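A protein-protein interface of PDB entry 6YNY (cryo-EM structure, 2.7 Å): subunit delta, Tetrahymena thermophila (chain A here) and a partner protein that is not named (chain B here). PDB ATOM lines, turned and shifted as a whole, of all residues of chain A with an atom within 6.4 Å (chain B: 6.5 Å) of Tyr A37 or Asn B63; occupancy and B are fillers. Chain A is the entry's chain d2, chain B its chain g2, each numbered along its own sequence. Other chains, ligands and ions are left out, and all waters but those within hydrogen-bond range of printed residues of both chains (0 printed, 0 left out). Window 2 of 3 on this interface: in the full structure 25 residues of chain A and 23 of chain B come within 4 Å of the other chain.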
ATOM      1  N   THR A  35      25.609  -9.080 -14.623  1.00  0.00           N
ATOM      2  CA  THR A  35      24.829  -8.117 -15.376  1.00  0.00           C
ATOM      3  C   THR A  35      25.803  -7.202 -16.110  1.00  0.00           C
ATOM      4  O   THR A  35      26.857  -6.859 -15.556  1.00  0.00           O
ATOM      5  CB  THR A  35      23.914  -7.297 -14.455  1.00  0.00           C
ATOM      6  OG1 THR A  35      23.097  -8.185 -13.682  1.00  0.00           O
ATOM      7  CG2 THR A  35      23.019  -6.371 -15.253  1.00  0.00           C
ATOM      8  N   PRO A  36      25.496  -6.799 -17.348  1.00  0.00           N
ATOM      9  CA  PRO A  36      26.483  -6.028 -18.122  1.00  0.00           C
ATOM     10  C   PRO A  36      27.004  -4.802 -17.396  1.00  0.00           C
ATOM     11  O   PRO A  36      28.136  -4.369 -17.653  1.00  0.00           O
ATOM     12  CB  PRO A  36      25.705  -5.643 -19.387  1.00  0.00           C
ATOM     13  CG  PRO A  36      24.661  -6.684 -19.518  1.00  0.00           C
ATOM     14  CD  PRO A  36      24.262  -7.031 -18.119  1.00  0.00           C
ATOM     15  N   TYR A  37      26.213  -4.230 -16.492  1.00  0.00           N
ATOM     16  CA  TYR A  37      26.578  -3.017 -15.774  1.00  0.00           C
ATOM     17  C   TYR A  37      27.062  -3.284 -14.357  1.00  0.00           C
ATOM     18  O   TYR A  37      27.536  -2.352 -13.698  1.00  0.00           O
ATOM     19  CB  TYR A  37      25.387  -2.056 -15.727  1.00  0.00           C
ATOM     20  CG  TYR A  37      24.652  -1.945 -17.040  1.00  0.00           C
ATOM     21  CD1 TYR A  37      23.571  -2.765 -17.323  1.00  0.00           C
ATOM     22  CD2 TYR A  37      25.043  -1.021 -17.999  1.00  0.00           C
ATOM     23  CE1 TYR A  37      22.897  -2.669 -18.522  1.00  0.00           C
ATOM     24  CE2 TYR A  37      24.376  -0.916 -19.201  1.00  0.00           C
ATOM     25  CZ  TYR A  37      23.306  -1.744 -19.457  1.00  0.00           C
ATOM     26  OH  TYR A  37      22.632  -1.644 -20.652  1.00  0.00           O
ATOM     27  N   LYS A  38      26.959  -4.518 -13.873  1.00  0.00           N
ATOM     28  CA  LYS A  38      27.418  -4.846 -12.532  1.00  0.00           C
ATOM     29  C   LYS A  38      27.462  -6.357 -12.379  1.00  0.00           C
ATOM     30  O   LYS A  38      26.656  -7.078 -12.972  1.00  0.00           O
ATOM     31  CB  LYS A  38      26.498  -4.237 -11.468  1.00  0.00           C
ATOM     32  CG  LYS A  38      27.135  -3.136 -10.639  1.00  0.00           C
ATOM     33  CD  LYS A  38      26.238  -2.732  -9.478  1.00  0.00           C
ATOM     34  CE  LYS A  38      26.213  -3.794  -8.388  1.00  0.00           C
ATOM     35  NZ  LYS A  38      25.461  -3.342  -7.186  1.00  0.00           N
ATOM     36  N   GLU A  39      28.413  -6.820 -11.573  1.00  0.00           N
ATOM     37  CA  GLU A  39      28.571  -8.230 -11.250  1.00  0.00           C
ATOM     38  C   GLU A  39      28.165  -8.436  -9.798  1.00  0.00           C
ATOM     39  O   GLU A  39      28.755  -7.836  -8.893  1.00  0.00           O
ATOM     40  CB  GLU A  39      30.011  -8.679 -11.491  1.00  0.00           C
ATOM     41  CG  GLU A  39      30.319 -10.093 -11.045  1.00  0.00           C
ATOM     42  CD  GLU A  39      31.649 -10.581 -11.580  1.00  0.00           C
ATOM     43  OE1 GLU A  39      31.717 -10.931 -12.776  1.00  0.00           O
ATOM     44  OE2 GLU A  39      32.631 -10.598 -10.810  1.00  0.00           O
ATOM     45  N   TYR A  40      27.159  -9.282  -9.579  1.00  0.00           N
ATOM     46  CA  TYR A  40      26.621  -9.501  -8.243  1.00  0.00           C
ATOM     47  C   TYR A  40      27.270 -10.683  -7.534  1.00  0.00           C
ATOM     48  O   TYR A  40      27.535 -10.611  -6.329  1.00  0.00           O
ATOM     49  CB  TYR A  40      25.108  -9.713  -8.325  1.00  0.00           C
ATOM     50  CG  TYR A  40      24.334  -8.449  -8.621  1.00  0.00           C
ATOM     51  CD1 TYR A  40      24.469  -7.800  -9.841  1.00  0.00           C
ATOM     52  CD2 TYR A  40      23.463  -7.910  -7.686  1.00  0.00           C
ATOM     53  CE1 TYR A  40      23.764  -6.645 -10.118  1.00  0.00           C
ATOM     54  CE2 TYR A  40      22.753  -6.755  -7.953  1.00  0.00           C
ATOM     55  CZ  TYR A  40      22.906  -6.127  -9.171  1.00  0.00           C
ATOM     56  OH  TYR A  40      22.202  -4.978  -9.442  1.00  0.00           O
ATOM     57  N   MET A 112      19.935  -8.990 -18.510  1.00  0.00           N
ATOM     58  CA  MET A 112      20.151  -7.636 -19.007  1.00  0.00           C
ATOM     59  C   MET A 112      20.283  -6.649 -17.853  1.00  0.00           C
ATOM     60  O   MET A 112      21.183  -5.802 -17.844  1.00  0.00           O
ATOM     61  CB  MET A 112      19.005  -7.237 -19.935  1.00  0.00           C
ATOM     62  CG  MET A 112      18.926  -8.061 -21.207  1.00  0.00           C
ATOM     63  SD  MET A 112      19.861  -7.346 -22.569  1.00  0.00           S
ATOM     64  CE  MET A 112      18.837  -5.932 -22.970  1.00  0.00           C
ATOM     65  N   ASP A 113      19.391  -6.743 -16.870  1.00  0.00           N
ATOM     66  CA  ASP A 113      19.442  -5.870 -15.706  1.00  0.00           C
ATOM     67  C   ASP A 113      18.705  -6.546 -14.560  1.00  0.00           C
ATOM     68  O   ASP A 113      17.906  -7.463 -14.768  1.00  0.00           O
ATOM     69  CB  ASP A 113      18.842  -4.494 -16.009  1.00  0.00           C
ATOM     70  CG  ASP A 113      19.220  -3.451 -14.973  1.00  0.00           C
ATOM     71  OD1 ASP A 113      19.242  -3.785 -13.769  1.00  0.00           O
ATOM     72  OD2 ASP A 113      19.506  -2.300 -15.364  1.00  0.00           O
ATOM     73  N   THR B  58      37.025   2.759 -16.560  1.00  0.00           N
ATOM     74  CA  THR B  58      37.561   1.635 -15.803  1.00  0.00           C
ATOM     75  C   THR B  58      36.542   1.121 -14.794  1.00  0.00           C
ATOM     76  O   THR B  58      36.395  -0.093 -14.611  1.00  0.00           O
ATOM     77  CB  THR B  58      38.854   2.044 -15.097  1.00  0.00           C
ATOM     78  OG1 THR B  58      38.620   3.212 -14.300  1.00  0.00           O
ATOM     79  CG2 THR B  58      39.946   2.332 -16.116  1.00  0.00           C
ATOM     80  N   SER B  59      35.826   2.032 -14.131  1.00  0.00           N
ATOM     81  CA  SER B  59      34.793   1.609 -13.191  1.00  0.00           C
ATOM     82  C   SER B  59      33.704   0.819 -13.901  1.00  0.00           C
ATOM     83  O   SER B  59      33.208  -0.184 -13.374  1.00  0.00           O
ATOM     84  CB  SER B  59      34.195   2.827 -12.487  1.00  0.00           C
ATOM     85  OG  SER B  59      33.176   2.442 -11.582  1.00  0.00           O
ATOM     86  N   ARG B  60      33.320   1.253 -15.102  1.00  0.00           N
ATOM     87  CA  ARG B  60      32.331   0.512 -15.874  1.00  0.00           C
ATOM     88  C   ARG B  60      32.932  -0.769 -16.435  1.00  0.00           C
ATOM     89  O   ARG B  60      32.261  -1.806 -16.491  1.00  0.00           O
ATOM     90  CB  ARG B  60      31.781   1.389 -16.998  1.00  0.00           C
ATOM     91  CG  ARG B  60      30.758   0.699 -17.881  1.00  0.00           C
ATOM     92  CD  ARG B  60      30.176   1.653 -18.911  1.00  0.00           C
ATOM     93  NE  ARG B  60      29.423   2.737 -18.286  1.00  0.00           N
ATOM     94  CZ  ARG B  60      28.788   3.695 -18.955  1.00  0.00           C
ATOM     95  NH1 ARG B  60      28.806   3.713 -20.281  1.00  0.00           N
ATOM     96  NH2 ARG B  60      28.129   4.637 -18.295  1.00  0.00           N
ATOM     97  N   LEU B  61      34.197  -0.716 -16.854  1.00  0.00           N
ATOM     98  CA  LEU B  61      34.858  -1.906 -17.377  1.00  0.00           C
ATOM     99  C   LEU B  61      34.982  -2.978 -16.302  1.00  0.00           C
ATOM    100  O   LEU B  61      34.618  -4.140 -16.522  1.00  0.00           O
ATOM    101  CB  LEU B  61      36.234  -1.534 -17.926  1.00  0.00           C
ATOM    102  CG  LEU B  61      37.158  -2.701 -18.282  1.00  0.00           C
ATOM    103  CD1 LEU B  61      36.481  -3.658 -19.242  1.00  0.00           C
ATOM    104  CD2 LEU B  61      38.459  -2.189 -18.874  1.00  0.00           C
ATOM    105  N   GLU B  62      35.490  -2.605 -15.125  1.00  0.00           N
ATOM    106  CA  GLU B  62      35.689  -3.591 -14.069  1.00  0.00           C
ATOM    107  C   GLU B  62      34.379  -4.241 -13.649  1.00  0.00           C
ATOM    108  O   GLU B  62      34.378  -5.385 -13.177  1.00  0.00           O
ATOM    109  CB  GLU B  62      36.365  -2.935 -12.865  1.00  0.00           C
ATOM    110  CG  GLU B  62      37.792  -2.482 -13.130  1.00  0.00           C
ATOM    111  CD  GLU B  62      38.731  -3.639 -13.409  1.00  0.00           C
ATOM    112  OE1 GLU B  62      39.752  -3.427 -14.096  1.00  0.00           O
ATOM    113  OE2 GLU B  62      38.447  -4.763 -12.942  1.00  0.00           O
ATOM    114  N   ASN B  63      33.258  -3.540 -13.809  1.00  0.00           N
ATOM    115  CA  ASN B  63      31.965  -4.078 -13.408  1.00  0.00           C
ATOM    116  C   ASN B  63      31.322  -4.927 -14.494  1.00  0.00           C
ATOM    117  O   ASN B  63      30.559  -5.847 -14.179  1.00  0.00           O
ATOM    118  CB  ASN B  63      31.016  -2.938 -13.028  1.00  0.00           C
ATOM    119  CG  ASN B  63      31.497  -2.160 -11.821  1.00  0.00           C
ATOM    120  OD1 ASN B  63      32.685  -2.161 -11.498  1.00  0.00           O
ATOM    121  ND2 ASN B  63      30.571  -1.492 -11.142  1.00  0.00           N
ATOM    122  N   GLY B  64      31.610  -4.640 -15.761  1.00  0.00           N
ATOM    123  CA  GLY B  64      30.997  -5.351 -16.864  1.00  0.00           C
ATOM    124  C   GLY B  64      31.917  -6.353 -17.530  1.00  0.00           C
ATOM    125  O   GLY B  64      31.472  -7.146 -18.366  1.00  0.00           O
ATOM    126  N   ARG B  65      33.199  -6.330 -17.175  1.00  0.00           N
ATOM    127  CA  ARG B  65      34.159  -7.213 -17.819  1.00  0.00           C
ATOM    128  C   ARG B  65      33.781  -8.673 -17.595  1.00  0.00           C
ATOM    129  O   ARG B  65      32.989  -9.014 -16.713  1.00  0.00           O
ATOM    130  CB  ARG B  65      35.572  -6.949 -17.299  1.00  0.00           C
ATOM    131  CG  ARG B  65      35.786  -7.331 -15.844  1.00  0.00           C
ATOM    132  CD  ARG B  65      37.176  -6.939 -15.360  1.00  0.00           C
ATOM    133  NE  ARG B  65      38.236  -7.461 -16.221  1.00  0.00           N
ATOM    134  CZ  ARG B  65      38.787  -6.796 -17.234  1.00  0.00           C
ATOM    135  NH1 ARG B  65      39.746  -7.365 -17.952  1.00  0.00           N
ATOM    136  NH2 ARG B  65      38.385  -5.569 -17.539  1.00  0.00           N
ATOM    137  N   ASN B  66      34.362  -9.539 -18.429  1.00  0.00           N
ATOM    138  CA  ASN B  66      34.159 -10.990 -18.356  1.00  0.00           C
ATOM    139  C   ASN B  66      32.684 -11.346 -18.188  1.00  0.00           C
ATOM    140  O   ASN B  66      32.340 -12.358 -17.572  1.00  0.00           O
ATOM    141  CB  ASN B  66      35.002 -11.615 -17.237  1.00  0.00           C
ATOM    142  CG  ASN B  66      34.575 -11.170 -15.848  1.00  0.00           C
ATOM    143  OD1 ASN B  66      33.394 -11.197 -15.503  1.00  0.00           O
ATOM    144  ND2 ASN B  66      35.546 -10.759 -15.039  1.00  0.00           N
ATOM    145  N   PHE B  67      31.801 -10.520 -18.743  1.00  0.00           N
ATOM    146  CA  PHE B  67      30.365 -10.766 -18.673  1.00  0.00           C
ATOM    147  C   PHE B  67      29.987 -11.773 -19.751  1.00  0.00           C
ATOM    148  O   PHE B  67      29.967 -11.442 -20.941  1.00  0.00           O
ATOM    149  CB  PHE B  67      29.585  -9.468 -18.846  1.00  0.00           C
ATOM    150  CG  PHE B  67      28.105  -9.670 -18.957  1.00  0.00           C
ATOM    151  CD1 PHE B  67      27.507  -9.836 -20.194  1.00  0.00           C
ATOM    152  CD2 PHE B  67      27.311  -9.701 -17.826  1.00  0.00           C
ATOM    153  CE1 PHE B  67      26.146 -10.026 -20.300  1.00  0.00           C
ATOM    154  CE2 PHE B  67      25.951  -9.893 -17.926  1.00  0.00           C
ATOM    155  CZ  PHE B  67      25.366 -10.055 -19.165  1.00  0.00           C
ATOM    156  N   VAL B 159      28.107   3.520 -24.080  1.00  0.00           N
ATOM    157  CA  VAL B 159      28.370   2.096 -24.240  1.00  0.00           C
ATOM    158  C   VAL B 159      27.455   1.339 -23.289  1.00  0.00           C
ATOM    159  O   VAL B 159      27.476   1.574 -22.075  1.00  0.00           O
ATOM    160  CB  VAL B 159      29.846   1.762 -23.970  1.00  0.00           C
ATOM    161  CG1 VAL B 159      30.108   0.284 -24.202  1.00  0.00           C
ATOM    162  CG2 VAL B 159      30.748   2.611 -24.850  1.00  0.00           C
ATOM    163  N   ASN B 160      26.651   0.433 -23.837  1.00  0.00           N
ATOM    164  CA  ASN B 160      25.759  -0.385 -23.029  1.00  0.00           C
ATOM    165  C   ASN B 160      25.392  -1.628 -23.825  1.00  0.00           C
ATOM    166  O   ASN B 160      25.503  -1.655 -25.054  1.00  0.00           O
ATOM    167  CB  ASN B 160      24.507   0.392 -22.611  1.00  0.00           C
ATOM    168  CG  ASN B 160      23.721   0.913 -23.794  1.00  0.00           C
ATOM    169  OD1 ASN B 160      24.290   1.269 -24.825  1.00  0.00           O
ATOM    170  ND2 ASN B 160      22.402   0.963 -23.650  1.00  0.00           N
ATOM    171  N   PHE B 161      24.952  -2.658 -23.106  1.00  0.00           N
ATOM    172  CA  PHE B 161      24.677  -3.935 -23.755  1.00  0.00           C
ATOM    173  C   PHE B 161      23.582  -3.827 -24.807  1.00  0.00           C
ATOM    174  O   PHE B 161      23.746  -4.414 -25.891  1.00  0.00           O
ATOM    175  CB  PHE B 161      24.314  -4.990 -22.705  1.00  0.00           C
ATOM    176  CG  PHE B 161      24.295  -6.388 -23.241  1.00  0.00           C
ATOM    177  CD1 PHE B 161      25.469  -7.108 -23.377  1.00  0.00           C
ATOM    178  CD2 PHE B 161      23.105  -6.983 -23.615  1.00  0.00           C
ATOM    179  CE1 PHE B 161      25.456  -8.394 -23.872  1.00  0.00           C
ATOM    180  CE2 PHE B 161      23.085  -8.270 -24.110  1.00  0.00           C
ATOM    181  CZ  PHE B 161      24.264  -8.976 -24.240  1.00  0.00           C
ATOM    182  N   PRO B 162      22.473  -3.122 -24.575  1.00  0.00           N
ATOM    183  CA  PRO B 162      21.479  -2.960 -25.648  1.00  0.00           C
ATOM    184  C   PRO B 162      22.076  -2.400 -26.925  1.00  0.00           C
ATOM    185  O   PRO B 162      21.756  -2.878 -28.020  1.00  0.00           O
ATOM    186  CB  PRO B 162      20.453  -2.003 -25.028  1.00  0.00           C
ATOM    187  CG  PRO B 162      20.586  -2.201 -23.565  1.00  0.00           C
ATOM    188  CD  PRO B 162      22.035  -2.485 -23.322  1.00  0.00           C
ATOM    189  N   THR B 163      22.943  -1.394 -26.814  1.00  0.00           N
ATOM    190  CA  THR B 163      23.594  -0.848 -27.999  1.00  0.00           C
ATOM    191  C   THR B 163      24.554  -1.863 -28.605  1.00  0.00           C
ATOM    192  O   THR B 163      24.535  -2.102 -29.817  1.00  0.00           O
ATOM    193  CB  THR B 163      24.331   0.443 -27.643  1.00  0.00           C
ATOM    194  OG1 THR B 163      23.415   1.375 -27.057  1.00  0.00           O
ATOM    195  CG2 THR B 163      24.952   1.062 -28.885  1.00  0.00           C
ATOM    196  N   TYR B 241      30.330  -6.239 -26.854  1.00  0.00           N
ATOM    197  CA  TYR B 241      30.206  -5.413 -25.659  1.00  0.00           C
ATOM    198  C   TYR B 241      31.529  -5.331 -24.910  1.00  0.00           C
ATOM    199  O   TYR B 241      31.903  -4.266 -24.404  1.00  0.00           O
ATOM    200  CB  TYR B 241      29.114  -5.973 -24.752  1.00  0.00           C
ATOM    201  CG  TYR B 241      28.911  -5.195 -23.474  1.00  0.00           C
ATOM    202  CD1 TYR B 241      28.099  -4.072 -23.444  1.00  0.00           C
ATOM    203  CD2 TYR B 241      29.530  -5.587 -22.295  1.00  0.00           C
ATOM    204  CE1 TYR B 241      27.907  -3.359 -22.279  1.00  0.00           C
ATOM    205  CE2 TYR B 241      29.345  -4.881 -21.124  1.00  0.00           C
ATOM    206  CZ  TYR B 241      28.534  -3.768 -21.121  1.00  0.00           C
ATOM    207  OH  TYR B 241      28.346  -3.061 -19.956  1.00  0.00           O
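OE1 of Glu A39 sits close to OD1 of Asn B66.
OH of Tyr B241 sits at hydrogen-bond distance from O of Pro A36 (2.7 Å).
O of Ser B59 lies close to OD1 of Asn B63.
C of Thr A35 touches CE2 of Phe B67, 3.2 Å away.
Gly B64 touches Pro A36 (CA to O, 3.1 Å).
Phe B67 touches Pro A36 (CE2 to N, 3.2 Å).
Pro A36 touches Phe B161 (CG to CB, 3.6 Å).
Tyr A37 touches Asn B63 (O to CB, 3.6 Å).
CB of Asn B160 touches OH of Tyr A37, 3.4 Å away.
Tyr A37 touches Phe B161.
Pro B162 touches Tyr A37.
Asn B63 touches Lys A38 (O to C, 3.6 Å).
Glu A39 touches Asn B63 (N to O, 3.5 Å).
Of chain B, only Asn B63 (3.6 Å), Asn B160 (3.4 Å), Phe B161 (3.5 Å) and Pro B162 (2.9 Å) come within 4 Å of Tyr A37.
Asn B63 touches three residues of chain A.
Of the printed residues of chain B, Glu A39 touches Asn B63 and Asn B66.
Printed residues of chain B within 4 Å of Met A112: Phe B161 (3.4 Å).
The nearest residue of chain A that does not touch Asn B63 is Thr A35 (4.1 Å).
Printed residues of chain B that touch a printed residue of chain A: Asn B63, Gly B64, Asn B66, Phe B67, Asn B160, Phe B161, Pro B162 and Tyr B241.
Hydrophobic or aromatic side chains of chain B within 4 Å of the printed part of chain A: Phe B67, Phe B161, Pro B162 and Tyr B241.
Of the 8 printed residues of chain A, 6 touch a printed residue of chain B.
Among the printed residues, 13 pairs touch across the chains.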
